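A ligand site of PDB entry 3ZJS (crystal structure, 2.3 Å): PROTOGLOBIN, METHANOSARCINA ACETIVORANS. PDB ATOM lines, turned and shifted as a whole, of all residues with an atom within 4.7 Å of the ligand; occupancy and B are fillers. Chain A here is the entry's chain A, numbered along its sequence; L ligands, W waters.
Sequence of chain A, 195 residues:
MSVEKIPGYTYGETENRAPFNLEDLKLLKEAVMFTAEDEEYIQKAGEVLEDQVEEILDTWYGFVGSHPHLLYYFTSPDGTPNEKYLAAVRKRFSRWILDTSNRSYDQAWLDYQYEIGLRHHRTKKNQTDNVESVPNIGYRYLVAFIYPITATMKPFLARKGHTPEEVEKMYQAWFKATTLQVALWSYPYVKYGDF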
ATOM      1  N   TYR A   9      -8.498  -5.713  18.836  1.00  0.00           N
ATOM      2  CA  TYR A   9      -7.526  -5.579  17.766  1.00  0.00           C
ATOM      3  C   TYR A   9      -8.077  -6.119  16.455  1.00  0.00           C
ATOM      4  O   TYR A   9      -8.259  -7.323  16.303  1.00  0.00           O
ATOM      5  CB  TYR A   9      -6.267  -6.322  18.115  1.00  0.00           C
ATOM      6  CG  TYR A   9      -5.217  -6.261  17.034  1.00  0.00           C
ATOM      7  CD1 TYR A   9      -4.520  -5.073  16.779  1.00  0.00           C
ATOM      8  CD2 TYR A   9      -4.868  -7.406  16.319  1.00  0.00           C
ATOM      9  CE1 TYR A   9      -3.499  -5.023  15.837  1.00  0.00           C
ATOM     10  CE2 TYR A   9      -3.856  -7.377  15.347  1.00  0.00           C
ATOM     11  CZ  TYR A   9      -3.173  -6.182  15.112  1.00  0.00           C
ATOM     12  OH  TYR A   9      -2.143  -6.165  14.195  1.00  0.00           O
ATOM     13  N   VAL A  64       2.528   8.879  30.803  1.00  0.00           N
ATOM     14  CA  VAL A  64       1.116   9.219  30.734  1.00  0.00           C
ATOM     15  C   VAL A  64       0.478   9.425  32.135  1.00  0.00           C
ATOM     16  O   VAL A  64      -0.095  10.413  32.398  1.00  0.00           O
ATOM     17  CB  VAL A  64       0.277   8.267  29.858  1.00  0.00           C
ATOM     18  CG1 VAL A  64      -1.177   8.562  30.001  1.00  0.00           C
ATOM     19  CG2 VAL A  64       0.624   8.419  28.412  1.00  0.00           C
ATOM     20  N   LEU A  70      -3.117  14.360  30.872  1.00  0.00           N
ATOM     21  CA  LEU A  70      -2.889  13.258  29.912  1.00  0.00           C
ATOM     22  C   LEU A  70      -3.542  11.920  30.295  1.00  0.00           C
ATOM     23  O   LEU A  70      -4.266  11.314  29.478  1.00  0.00           O
ATOM     24  CB  LEU A  70      -1.381  13.089  29.595  1.00  0.00           C
ATOM     25  CG  LEU A  70      -0.663  14.323  29.014  1.00  0.00           C
ATOM     26  CD1 LEU A  70       0.799  14.061  28.646  1.00  0.00           C
ATOM     27  CD2 LEU A  70      -1.435  14.924  27.804  1.00  0.00           C
ATOM     28  N   TYR A  73      -7.485  11.134  29.699  1.00  0.00           N
ATOM     29  CA  TYR A  73      -8.169  10.525  28.558  1.00  0.00           C
ATOM     30  C   TYR A  73      -8.449   9.025  28.754  1.00  0.00           C
ATOM     31  O   TYR A  73      -9.295   8.450  28.065  1.00  0.00           O
ATOM     32  CB  TYR A  73      -7.411  10.800  27.258  1.00  0.00           C
ATOM     33  CG  TYR A  73      -7.373  12.273  26.924  1.00  0.00           C
ATOM     34  CD1 TYR A  73      -8.497  12.914  26.398  1.00  0.00           C
ATOM     35  CD2 TYR A  73      -6.244  13.030  27.194  1.00  0.00           C
ATOM     36  CE1 TYR A  73      -8.489  14.296  26.158  1.00  0.00           C
ATOM     37  CE2 TYR A  73      -6.245  14.410  26.994  1.00  0.00           C
ATOM     38  CZ  TYR A  73      -7.366  15.034  26.485  1.00  0.00           C
ATOM     39  OH  TYR A  73      -7.344  16.383  26.239  1.00  0.00           O
ATOM     40  N   PHE A  74      -7.815   8.431  29.768  1.00  0.00           N
ATOM     41  CA  PHE A  74      -8.174   7.092  30.251  1.00  0.00           C
ATOM     42  C   PHE A  74      -9.088   7.077  31.501  1.00  0.00           C
ATOM     43  O   PHE A  74      -9.254   6.025  32.110  1.00  0.00           O
ATOM     44  CB  PHE A  74      -6.908   6.285  30.593  1.00  0.00           C
ATOM     45  CG  PHE A  74      -6.056   5.959  29.396  1.00  0.00           C
ATOM     46  CD1 PHE A  74      -5.062   6.848  28.958  1.00  0.00           C
ATOM     47  CD2 PHE A  74      -6.241   4.778  28.690  1.00  0.00           C
ATOM     48  CE1 PHE A  74      -4.254   6.534  27.840  1.00  0.00           C
ATOM     49  CE2 PHE A  74      -5.442   4.467  27.570  1.00  0.00           C
ATOM     50  CZ  PHE A  74      -4.445   5.338  27.149  1.00  0.00           C
ATOM     51  N   TYR A  85      -9.598  -0.042  30.960  1.00  0.00           N
ATOM     52  CA  TYR A  85      -9.362   0.752  29.763  1.00  0.00           C
ATOM     53  C   TYR A  85      -7.861   0.783  29.461  1.00  0.00           C
ATOM     54  O   TYR A  85      -7.433   0.461  28.346  1.00  0.00           O
ATOM     55  CB  TYR A  85      -9.907   2.166  29.989  1.00  0.00           C
ATOM     56  CG  TYR A  85     -10.076   3.025  28.748  1.00  0.00           C
ATOM     57  CD1 TYR A  85     -10.015   2.482  27.469  1.00  0.00           C
ATOM     58  CD2 TYR A  85     -10.284   4.399  28.858  1.00  0.00           C
ATOM     59  CE1 TYR A  85     -10.218   3.260  26.356  1.00  0.00           C
ATOM     60  CE2 TYR A  85     -10.481   5.198  27.742  1.00  0.00           C
ATOM     61  CZ  TYR A  85     -10.422   4.632  26.499  1.00  0.00           C
ATOM     62  OH  TYR A  85     -10.592   5.415  25.385  1.00  0.00           O
ATOM     63  N   VAL A  89      -6.099  -1.235  26.058  1.00  0.00           N
ATOM     64  CA  VAL A  89      -5.362  -0.375  25.123  1.00  0.00           C
ATOM     65  C   VAL A  89      -3.878  -0.699  25.108  1.00  0.00           C
ATOM     66  O   VAL A  89      -3.254  -0.741  24.044  1.00  0.00           O
ATOM     67  CB  VAL A  89      -5.550   1.110  25.487  1.00  0.00           C
ATOM     68  CG1 VAL A  89      -4.630   2.002  24.674  1.00  0.00           C
ATOM     69  CG2 VAL A  89      -7.002   1.539  25.305  1.00  0.00           C
ATOM     70  N   ARG A  92      -3.146  -3.439  22.765  1.00  0.00           N
ATOM     71  CA  ARG A  92      -3.243  -3.011  21.370  1.00  0.00           C
ATOM     72  C   ARG A  92      -2.098  -2.054  20.993  1.00  0.00           C
ATOM     73  O   ARG A  92      -1.607  -2.091  19.863  1.00  0.00           O
ATOM     74  CB  ARG A  92      -4.604  -2.394  21.064  1.00  0.00           C
ATOM     75  CG  ARG A  92      -5.769  -3.367  21.248  1.00  0.00           C
ATOM     76  CD  ARG A  92      -6.989  -2.852  20.518  1.00  0.00           C
ATOM     77  NE  ARG A  92      -7.485  -1.602  21.096  1.00  0.00           N
ATOM     78  CZ  ARG A  92      -8.247  -1.553  22.179  1.00  0.00           C
ATOM     79  NH1 ARG A  92      -8.535  -2.684  22.829  1.00  0.00           N
ATOM     80  NH2 ARG A  92      -8.662  -0.382  22.669  1.00  0.00           N
ATOM     81  N   PHE A  93      -1.605  -1.315  21.982  1.00  0.00           N
ATOM     82  CA  PHE A  93      -0.494  -0.410  21.774  1.00  0.00           C
ATOM     83  C   PHE A  93       0.782  -1.207  21.529  1.00  0.00           C
ATOM     84  O   PHE A  93       1.541  -0.948  20.581  1.00  0.00           O
ATOM     85  CB  PHE A  93      -0.310   0.494  23.000  1.00  0.00           C
ATOM     86  CG  PHE A  93       0.646   1.649  22.772  1.00  0.00           C
ATOM     87  CD1 PHE A  93       2.011   1.506  23.007  1.00  0.00           C
ATOM     88  CD2 PHE A  93       0.168   2.899  22.385  1.00  0.00           C
ATOM     89  CE1 PHE A  93       2.877   2.603  22.899  1.00  0.00           C
ATOM     90  CE2 PHE A  93       1.019   3.968  22.211  1.00  0.00           C
ATOM     91  CZ  PHE A  93       2.381   3.829  22.467  1.00  0.00           C
ATOM     92  N   TRP A  96       0.907  -2.473  18.068  1.00  0.00           N
ATOM     93  CA  TRP A  96       1.201  -1.394  17.102  1.00  0.00           C
ATOM     94  C   TRP A  96       2.716  -1.161  16.983  1.00  0.00           C
ATOM     95  O   TRP A  96       3.212  -0.891  15.892  1.00  0.00           O
ATOM     96  CB  TRP A  96       0.485  -0.101  17.516  1.00  0.00           C
ATOM     97  CG  TRP A  96       0.976   1.111  16.836  1.00  0.00           C
ATOM     98  CD1 TRP A  96       0.584   1.585  15.613  1.00  0.00           C
ATOM     99  CD2 TRP A  96       1.968   2.026  17.310  1.00  0.00           C
ATOM    100  NE1 TRP A  96       1.259   2.731  15.308  1.00  0.00           N
ATOM    101  CE2 TRP A  96       2.166   2.985  16.305  1.00  0.00           C
ATOM    102  CE3 TRP A  96       2.742   2.091  18.485  1.00  0.00           C
ATOM    103  CZ2 TRP A  96       3.091   4.041  16.437  1.00  0.00           C
ATOM    104  CZ3 TRP A  96       3.685   3.127  18.605  1.00  0.00           C
ATOM    105  CH2 TRP A  96       3.826   4.100  17.588  1.00  0.00           C
ATOM    106  N   TYR A 112      -6.281   0.258   8.721  1.00  0.00           N
ATOM    107  CA  TYR A 112      -6.148   0.276  10.173  1.00  0.00           C
ATOM    108  C   TYR A 112      -5.723   1.632  10.780  1.00  0.00           C
ATOM    109  O   TYR A 112      -6.124   1.974  11.886  1.00  0.00           O
ATOM    110  CB  TYR A 112      -5.341  -0.917  10.719  1.00  0.00           C
ATOM    111  CG  TYR A 112      -5.722  -1.261  12.152  1.00  0.00           C
ATOM    112  CD1 TYR A 112      -6.992  -1.762  12.450  1.00  0.00           C
ATOM    113  CD2 TYR A 112      -4.809  -1.078  13.194  1.00  0.00           C
ATOM    114  CE1 TYR A 112      -7.303  -2.174  13.763  1.00  0.00           C
ATOM    115  CE2 TYR A 112      -5.129  -1.436  14.510  1.00  0.00           C
ATOM    116  CZ  TYR A 112      -6.389  -1.945  14.797  1.00  0.00           C
ATOM    117  OH  TYR A 112      -6.698  -2.218  16.109  1.00  0.00           O
ATOM    118  N   ILE A 116      -7.490   3.537  13.738  1.00  0.00           N
ATOM    119  CA  ILE A 116      -6.829   4.056  14.933  1.00  0.00           C
ATOM    120  C   ILE A 116      -7.094   5.553  15.118  1.00  0.00           C
ATOM    121  O   ILE A 116      -7.238   6.023  16.245  1.00  0.00           O
ATOM    122  CB  ILE A 116      -5.339   3.838  14.919  1.00  0.00           C
ATOM    123  CG1 ILE A 116      -5.020   2.347  15.062  1.00  0.00           C
ATOM    124  CG2 ILE A 116      -4.703   4.617  16.087  1.00  0.00           C
ATOM    125  CD1 ILE A 116      -3.543   2.008  14.847  1.00  0.00           C
ATOM    126  N   ARG A 119     -10.565   5.936  16.658  1.00  0.00           N
ATOM    127  CA  ARG A 119     -10.655   5.501  18.045  1.00  0.00           C
ATOM    128  C   ARG A 119     -10.092   6.555  19.018  1.00  0.00           C
ATOM    129  O   ARG A 119     -10.396   6.513  20.218  1.00  0.00           O
ATOM    130  CB  ARG A 119      -9.912   4.189  18.225  1.00  0.00           C
ATOM    131  CG  ARG A 119     -10.530   3.039  17.467  1.00  0.00           C
ATOM    132  CD  ARG A 119      -9.803   1.710  17.767  1.00  0.00           C
ATOM    133  NE  ARG A 119     -10.506   0.621  17.091  1.00  0.00           N
ATOM    134  CZ  ARG A 119     -10.297  -0.686  17.282  1.00  0.00           C
ATOM    135  NH1 ARG A 119      -9.342  -1.114  18.086  1.00  0.00           N
ATOM    136  NH2 ARG A 119     -11.029  -1.546  16.613  1.00  0.00           N
ATOM    137  N   HIS A 120      -9.200   7.423  18.536  1.00  0.00           N
ATOM    138  CA  HIS A 120      -8.735   8.561  19.314  1.00  0.00           C
ATOM    139  C   HIS A 120      -9.766   9.691  19.250  1.00  0.00           C
ATOM    140  O   HIS A 120      -9.924  10.438  20.208  1.00  0.00           O
ATOM    141  CB  HIS A 120      -7.378   9.063  18.781  1.00  0.00           C
ATOM    142  CG  HIS A 120      -6.198   8.269  19.255  1.00  0.00           C
ATOM    143  ND1 HIS A 120      -5.773   7.115  18.623  1.00  0.00           N
ATOM    144  CD2 HIS A 120      -5.347   8.455  20.292  1.00  0.00           C
ATOM    145  CE1 HIS A 120      -4.763   6.593  19.295  1.00  0.00           C
ATOM    146  NE2 HIS A 120      -4.480   7.392  20.311  1.00  0.00           N
ATOM    147  N   LYS A 124     -15.183   7.044  17.411  1.00  0.00           N
ATOM    148  CA  LYS A 124     -15.132   5.665  17.893  1.00  0.00           C
ATOM    149  C   LYS A 124     -14.429   5.481  19.232  1.00  0.00           C
ATOM    150  O   LYS A 124     -14.225   4.348  19.668  1.00  0.00           O
ATOM    151  CB  LYS A 124     -14.489   4.769  16.836  1.00  0.00           C
ATOM    152  CG  LYS A 124     -15.452   4.299  15.749  1.00  0.00           C
ATOM    153  CD  LYS A 124     -14.870   3.121  14.979  1.00  0.00           C
ATOM    154  CE  LYS A 124     -14.818   1.870  15.834  1.00  0.00           C
ATOM    155  NZ  LYS A 124     -14.352   0.690  15.065  1.00  0.00           N
ATOM    156  N   LYS A 125     -14.038   6.568  19.889  1.00  0.00           N
ATOM    157  CA  LYS A 125     -13.383   6.416  21.193  1.00  0.00           C
ATOM    158  C   LYS A 125     -14.329   5.727  22.178  1.00  0.00           C
ATOM    159  O   LYS A 125     -15.539   6.013  22.190  1.00  0.00           O
ATOM    160  CB  LYS A 125     -12.868   7.754  21.743  1.00  0.00           C
ATOM    161  CG  LYS A 125     -11.972   7.594  22.979  1.00  0.00           C
ATOM    162  CD  LYS A 125     -11.631   8.960  23.599  1.00  0.00           C
ATOM    163  CE  LYS A 125     -10.659   8.835  24.757  1.00  0.00           C
ATOM    164  NZ  LYS A 125     -11.308   8.372  26.019  1.00  0.00           N
ATOM    165  N   ASN A 126     -13.794   4.846  23.014  1.00  0.00           N
ATOM    166  CA  ASN A 126     -14.566   4.204  24.082  1.00  0.00           C
ATOM    167  C   ASN A 126     -15.531   3.068  23.677  1.00  0.00           C
ATOM    168  O   ASN A 126     -16.051   2.339  24.526  1.00  0.00           O
ATOM    169  CB  ASN A 126     -15.483   5.233  24.772  1.00  0.00           C
ATOM    170  CG  ASN A 126     -14.701   6.378  25.432  1.00  0.00           C
ATOM    171  OD1 ASN A 126     -13.596   6.171  25.955  1.00  0.00           O
ATOM    172  ND2 ASN A 126     -15.279   7.566  25.431  1.00  0.00           N
ATOM    173  N   THR A 128     -14.487   0.444  21.334  1.00  0.00           N
ATOM    174  CA  THR A 128     -13.723  -0.792  21.284  1.00  0.00           C
ATOM    175  C   THR A 128     -13.789  -1.570  22.596  1.00  0.00           C
ATOM    176  O   THR A 128     -14.053  -2.778  22.593  1.00  0.00           O
ATOM    177  CB  THR A 128     -12.246  -0.545  20.836  1.00  0.00           C
ATOM    178  OG1 THR A 128     -12.261   0.089  19.546  1.00  0.00           O
ATOM    179  CG2 THR A 128     -11.467  -1.855  20.779  1.00  0.00           C
ATOM    180  N   ASP A 129     -13.565  -0.892  23.710  1.00  0.00           N
ATOM    181  CA  ASP A 129     -13.478  -1.579  24.993  1.00  0.00           C
ATOM    182  C   ASP A 129     -14.794  -1.450  25.791  1.00  0.00           C
ATOM    183  O   ASP A 129     -14.929  -2.000  26.883  1.00  0.00           O
ATOM    184  CB  ASP A 129     -12.289  -1.052  25.801  1.00  0.00           C
ATOM    185  CG  ASP A 129     -10.956  -1.202  25.055  1.00  0.00           C
ATOM    186  OD1 ASP A 129     -10.541  -2.356  24.797  1.00  0.00           O
ATOM    187  OD2 ASP A 129     -10.300  -0.172  24.753  1.00  0.00           O
ATOM    188  N   ILE A 137     -10.112  12.770  22.304  1.00  0.00           N
ATOM    189  CA  ILE A 137      -8.765  13.249  22.612  1.00  0.00           C
ATOM    190  C   ILE A 137      -8.467  14.436  21.702  1.00  0.00           C
ATOM    191  O   ILE A 137      -8.485  14.289  20.467  1.00  0.00           O
ATOM    192  CB  ILE A 137      -7.737  12.146  22.447  1.00  0.00           C
ATOM    193  CG1 ILE A 137      -8.196  10.919  23.216  1.00  0.00           C
ATOM    194  CG2 ILE A 137      -6.313  12.612  22.879  1.00  0.00           C
ATOM    195  CD1 ILE A 137      -7.307   9.677  23.058  1.00  0.00           C
ATOM    196  N   TYR A 141      -2.903  17.049  21.156  1.00  0.00           N
ATOM    197  CA  TYR A 141      -2.059  16.106  21.830  1.00  0.00           C
ATOM    198  C   TYR A 141      -1.599  14.937  20.943  1.00  0.00           C
ATOM    199  O   TYR A 141      -0.532  14.379  21.167  1.00  0.00           O
ATOM    200  CB  TYR A 141      -2.707  15.639  23.133  1.00  0.00           C
ATOM    201  CG  TYR A 141      -2.911  16.760  24.149  1.00  0.00           C
ATOM    202  CD1 TYR A 141      -1.837  17.396  24.766  1.00  0.00           C
ATOM    203  CD2 TYR A 141      -4.197  17.162  24.487  1.00  0.00           C
ATOM    204  CE1 TYR A 141      -2.058  18.428  25.707  1.00  0.00           C
ATOM    205  CE2 TYR A 141      -4.426  18.177  25.389  1.00  0.00           C
ATOM    206  CZ  TYR A 141      -3.369  18.791  26.016  1.00  0.00           C
ATOM    207  OH  TYR A 141      -3.682  19.814  26.877  1.00  0.00           O
ATOM    208  N   LEU A 142      -2.398  14.539  19.964  1.00  0.00           N
ATOM    209  CA  LEU A 142      -1.917  13.522  19.000  1.00  0.00           C
ATOM    210  C   LEU A 142      -0.642  14.026  18.349  1.00  0.00           C
ATOM    211  O   LEU A 142       0.335  13.306  18.284  1.00  0.00           O
ATOM    212  CB  LEU A 142      -2.955  13.211  17.897  1.00  0.00           C
ATOM    213  CG  LEU A 142      -3.825  12.008  18.220  1.00  0.00           C
ATOM    214  CD1 LEU A 142      -4.576  12.341  19.499  1.00  0.00           C
ATOM    215  CD2 LEU A 142      -4.786  11.711  17.067  1.00  0.00           C
ATOM    216  N   PHE A 145       2.347  14.291  20.840  1.00  0.00           N
ATOM    217  CA  PHE A 145       2.902  13.001  21.269  1.00  0.00           C
ATOM    218  C   PHE A 145       3.940  12.393  20.327  1.00  0.00           C
ATOM    219  O   PHE A 145       4.618  11.419  20.678  1.00  0.00           O
ATOM    220  CB  PHE A 145       1.819  11.968  21.553  1.00  0.00           C
ATOM    221  CG  PHE A 145       1.362  11.951  22.978  1.00  0.00           C
ATOM    222  CD1 PHE A 145       1.302  13.142  23.719  1.00  0.00           C
ATOM    223  CD2 PHE A 145       0.822  10.788  23.541  1.00  0.00           C
ATOM    224  CE1 PHE A 145       0.742  13.149  25.005  1.00  0.00           C
ATOM    225  CE2 PHE A 145       0.305  10.791  24.816  1.00  0.00           C
ATOM    226  CZ  PHE A 145       0.263  11.968  25.557  1.00  0.00           C
ATOM    227  N   ILE A 146       4.029  12.909  19.105  1.00  0.00           N
ATOM    228  CA  ILE A 146       5.129  12.515  18.224  1.00  0.00           C
ATOM    229  C   ILE A 146       6.447  12.631  18.976  1.00  0.00           C
ATOM    230  O   ILE A 146       7.287  11.732  18.908  1.00  0.00           O
ATOM    231  CB  ILE A 146       5.154  13.335  16.904  1.00  0.00           C
ATOM    232  CG1 ILE A 146       3.860  13.056  16.087  1.00  0.00           C
ATOM    233  CG2 ILE A 146       6.382  12.946  16.068  1.00  0.00           C
ATOM    234  CD1 ILE A 146       3.562  14.069  14.901  1.00  0.00           C
ATOM    235  N   ILE A 149       6.824   9.997  21.937  1.00  0.00           N
ATOM    236  CA  ILE A 149       6.774   8.647  21.400  1.00  0.00           C
ATOM    237  C   ILE A 149       8.106   8.256  20.731  1.00  0.00           C
ATOM    238  O   ILE A 149       8.621   7.139  20.931  1.00  0.00           O
ATOM    239  CB  ILE A 149       5.615   8.465  20.390  1.00  0.00           C
ATOM    240  CG1 ILE A 149       4.304   8.234  21.135  1.00  0.00           C
ATOM    241  CG2 ILE A 149       5.905   7.282  19.443  1.00  0.00           C
ATOM    242  CD1 ILE A 149       4.215   6.828  21.766  1.00  0.00           C
ATOM    243  N   THR A 178       6.180   7.350  12.877  1.00  0.00           N
ATOM    244  CA  THR A 178       5.250   7.880  13.866  1.00  0.00           C
ATOM    245  C   THR A 178       4.646   9.160  13.304  1.00  0.00           C
ATOM    246  O   THR A 178       3.428   9.347  13.391  1.00  0.00           O
ATOM    247  CB  THR A 178       5.983   8.226  15.179  1.00  0.00           C
ATOM    248  OG1 THR A 178       6.598   7.051  15.711  1.00  0.00           O
ATOM    249  CG2 THR A 178       5.015   8.768  16.216  1.00  0.00           C
ATOM    250  N   VAL A 182       0.598   9.592  12.625  1.00  0.00           N
ATOM    251  CA  VAL A 182      -0.176  10.655  13.267  1.00  0.00           C
ATOM    252  C   VAL A 182      -0.786  11.563  12.203  1.00  0.00           C
ATOM    253  O   VAL A 182      -1.884  12.052  12.381  1.00  0.00           O
ATOM    254  CB  VAL A 182       0.661  11.499  14.239  1.00  0.00           C
ATOM    255  CG1 VAL A 182      -0.142  12.728  14.697  1.00  0.00           C
ATOM    256  CG2 VAL A 182       1.113  10.656  15.442  1.00  0.00           C
ATOM    257  N   TRP A 185      -3.845   9.859  11.017  1.00  0.00           N
ATOM    258  CA  TRP A 185      -4.853   9.779  12.071  1.00  0.00           C
ATOM    259  C   TRP A 185      -5.619  11.072  12.202  1.00  0.00           C
ATOM    260  O   TRP A 185      -6.637  11.111  12.859  1.00  0.00           O
ATOM    261  CB  TRP A 185      -4.246   9.427  13.420  1.00  0.00           C
ATOM    262  CG  TRP A 185      -3.514   8.096  13.474  1.00  0.00           C
ATOM    263  CD1 TRP A 185      -3.483   7.127  12.511  1.00  0.00           C
ATOM    264  CD2 TRP A 185      -2.784   7.591  14.583  1.00  0.00           C
ATOM    265  NE1 TRP A 185      -2.754   6.048  12.953  1.00  0.00           N
ATOM    266  CE2 TRP A 185      -2.291   6.321  14.214  1.00  0.00           C
ATOM    267  CE3 TRP A 185      -2.501   8.083  15.862  1.00  0.00           C
ATOM    268  CZ2 TRP A 185      -1.476   5.562  15.054  1.00  0.00           C
ATOM    269  CZ3 TRP A 185      -1.712   7.313  16.714  1.00  0.00           C
ATOM    270  CH2 TRP A 185      -1.191   6.077  16.297  1.00  0.00           C
HETATM  271  C1  LIG L   1      -5.287   4.076  21.642  1.00  0.00           C
HETATM  272  C2  LIG L   1      -0.868   5.097  19.903  1.00  0.00           C
HETATM  273  C3  LIG L   1      -1.675   9.739  20.923  1.00  0.00           C
HETATM  274  C4  LIG L   1      -4.512   7.973  24.486  1.00  0.00           C
HETATM  275  C5  LIG L   1      -4.071   3.885  21.014  1.00  0.00           C
HETATM  276  C6  LIG L   1      -3.606   2.719  20.270  1.00  0.00           C
HETATM  277  C7  LIG L   1      -2.384   3.012  19.789  1.00  0.00           C
HETATM  278  C8  LIG L   1      -2.019   4.366  20.218  1.00  0.00           C
HETATM  279  C9  LIG L   1      -1.514   2.075  18.920  1.00  0.00           C
HETATM  280  C10 LIG L   1      -4.359   1.355  20.101  1.00  0.00           C
HETATM  281  C11 LIG L   1      -5.236   1.410  18.850  1.00  0.00           C
HETATM  282  C12 LIG L   1      -6.043   0.141  18.652  1.00  0.00           C
HETATM  283  O1  LIG L   1      -5.525  -0.841  18.031  1.00  0.00           O
HETATM  284  O2  LIG L   1      -7.228   0.149  19.050  1.00  0.00           O
HETATM  285  C13 LIG L   1      -0.704   6.479  19.889  1.00  0.00           C
HETATM  286  C14 LIG L   1       0.355   7.302  19.297  1.00  0.00           C
HETATM  287  C15 LIG L   1       0.116   8.592  19.568  1.00  0.00           C
HETATM  288  C16 LIG L   1      -1.095   8.630  20.356  1.00  0.00           C
HETATM  289  C17 LIG L   1       1.554   6.763  18.474  1.00  0.00           C
HETATM  290  C18 LIG L   1       0.899   9.854  19.121  1.00  0.00           C
HETATM  291  C19 LIG L   1       2.105   9.752  18.549  1.00  0.00           C
HETATM  292  C20 LIG L   1      -2.430   9.664  22.079  1.00  0.00           C
HETATM  293  C21 LIG L   1      -2.719  10.726  23.032  1.00  0.00           C
HETATM  294  C22 LIG L   1      -3.471  10.221  24.006  1.00  0.00           C
HETATM  295  C23 LIG L   1      -3.733   8.834  23.713  1.00  0.00           C
HETATM  296  C24 LIG L   1      -2.225  12.189  22.925  1.00  0.00           C
HETATM  297  C25 LIG L   1      -3.916  10.941  25.278  1.00  0.00           C
HETATM  298  C26 LIG L   1      -3.489  10.372  26.417  1.00  0.00           C
HETATM  299  C27 LIG L   1      -5.159   6.859  23.979  1.00  0.00           C
HETATM  300  C28 LIG L   1      -6.446   6.325  24.381  1.00  0.00           C
HETATM  301  C29 LIG L   1      -6.724   5.164  23.419  1.00  0.00           C
HETATM  302  C30 LIG L   1      -5.548   5.066  22.571  1.00  0.00           C
HETATM  303  C31 LIG L   1      -7.407   6.848  25.468  1.00  0.00           C
HETATM  304  C32 LIG L   1      -7.964   4.261  23.378  1.00  0.00           C
HETATM  305  C33 LIG L   1      -8.951   4.917  22.429  1.00  0.00           C
HETATM  306  C34 LIG L   1     -10.191   4.070  22.350  1.00  0.00           C
HETATM  307  O3  LIG L   1     -11.035   4.177  23.278  1.00  0.00           O
HETATM  308  O4  LIG L   1     -10.294   3.227  21.433  1.00  0.00           O
HETATM  309  N1  LIG L   1      -3.106   4.870  20.899  1.00  0.00           N
HETATM  310  N2  LIG L   1      -1.557   7.338  20.512  1.00  0.00           N
HETATM  311  N3  LIG L   1      -3.103   8.539  22.510  1.00  0.00           N
HETATM  312  N4  LIG L   1      -4.681   6.071  22.942  1.00  0.00           N
HETATM  313 FE1  LIG L   1      -3.096   6.714  21.672  1.00  0.00          FE
HETATM  314  O   HOH W   1     -12.045   1.465  23.875  1.00  0.00           O
HETATM  315  O   HOH W   2      -7.965   1.730  21.086  1.00  0.00           O
HETATM  316  O   HOH W   3      -2.800  -1.483  17.368  1.00  0.00           O
HETATM  317  O   HOH W   4     -12.653   2.709  20.456  1.00  0.00           O
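NZ of Lys 125 is in hydrogen-bond range of OH of Tyr 85 (3.1 Å). NZ of Lys 125 lies within hydrogen-bond range of O of Tyr 73 (2.9 Å). A ring nitrogen (ND1) of His 120 lies within hydrogen-bond range of the backbone carbonyl oxygen of Ile 116, at 3.0 Å. The side-chain amide oxygen (OD1) of Asn 126 is in hydrogen-bond range of the side-chain hydroxyl (OH) of Tyr 85, at 3.1 Å. NE of Arg 119 is in hydrogen-bond range of OG1 of Thr 128 (3.1 Å). The guanidinium group (NH2) of Arg 92 lies within salt-bridge range of the side-chain carboxylate (OD2) of Asp 129, 2.7 Å away. The backbone carbonyl oxygen (O) of His 120 is in hydrogen-bond range of the backbone NH (N) of Ile 137 (3.1 Å). NZ of Lys 125 lies within hydrogen-bond range of OD1 of Asn 126 (3.2 Å).
O3 of the ligand lies within hydrogen-bond range of OH of Tyr 85, at 2.5 Å. The guanidinium group of Arg 92 lies within salt-bridge range of an oxygen (O2) of the ligand. FE1 of the ligand is bound by NE2 of His 120. The backbone NH (N) of Asn 126 lies within hydrogen-bond range of an oxygen (O3) of the ligand (2.9 Å). NH1 of Arg 119 lies within salt-bridge range of O2 of the ligand. The side-chain hydroxyl (OH) of Tyr 112 is in hydrogen-bond range of an oxygen (O1) of the ligand, at 2.6 Å.
Water W4 lies within hydrogen-bond range of the backbone carbonyl oxygen (O) of Lys 124, an oxygen (O4) of the ligand and the side-chain hydroxyl (OG1) of Thr 128. Water W2 bridges an oxygen (O2) of the ligand and the guanidinium group of Arg 92. Water W3 lies within hydrogen-bond range of the backbone carbonyl oxygen of Arg 92 (2.8 Å) and an oxygen (O1) of the ligand (2.9 Å). Water W1 bridges the side-chain carboxylate of Asp 129 (2.5 Å) and an oxygen (O3) of the ligand (3.0 Å).
O of Leu 70 touches C26 of the ligand, at 3.3 Å. Tyr 73 touches the ligand (O to C31, 3.6 Å). CZ of Phe 74 touches C28 of the ligand, 3.6 Å away. Val 89 touches the ligand. Phe 93 touches the ligand (CE2 to C2, 3.2 Å). CB of Trp 96 touches C9 of the ligand (3.3 Å). Ile 116 touches the ligand (CG1 to C11, 3.9 Å). CG of Lys 125 touches O3 of the ligand, 3.6 Å away. Ile 137 touches the ligand (CD1 to C4, 3.6 Å). Tyr 141 touches the ligand. O of Leu 142 touches C18 of the ligand, 3.6 Å away. Phe 145 touches the ligand (CB to C18, 3.4 Å). Ile 146 touches the ligand. Ile 149 touches the ligand. Thr 178 touches the ligand. Val 182 touches the ligand (CG2 to C19, 3.4 Å). CZ3 of Trp 185 touches C14 of the ligand, at 3.3 Å. Hydrophobic or aromatic side chains within 4 Å of the ligand: Tyr 73, Phe 74, Tyr 85, Val 89, Phe 93, Trp 96, Tyr 112, Ile 116, His 120, Ile 137, Tyr 141, Phe 145, Ile 149, Val 182 and Trp 185. 23 residues have an atom within 4 Å of the ligand: Leu 70, Tyr 73, Phe 74, Tyr 85, Val 89, Arg 92, Phe 93, Trp 96, Tyr 112, Ile 116, Arg 119, His 120, Lys 125, Asn 126, Ile 137, Tyr 141, Leu 142, Phe 145, Ile 146, Ile 149, Thr 178, Val 182 and Trp 185. The nearest printed residue that does not touch the ligand is Thr 128 (4.2 Å).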
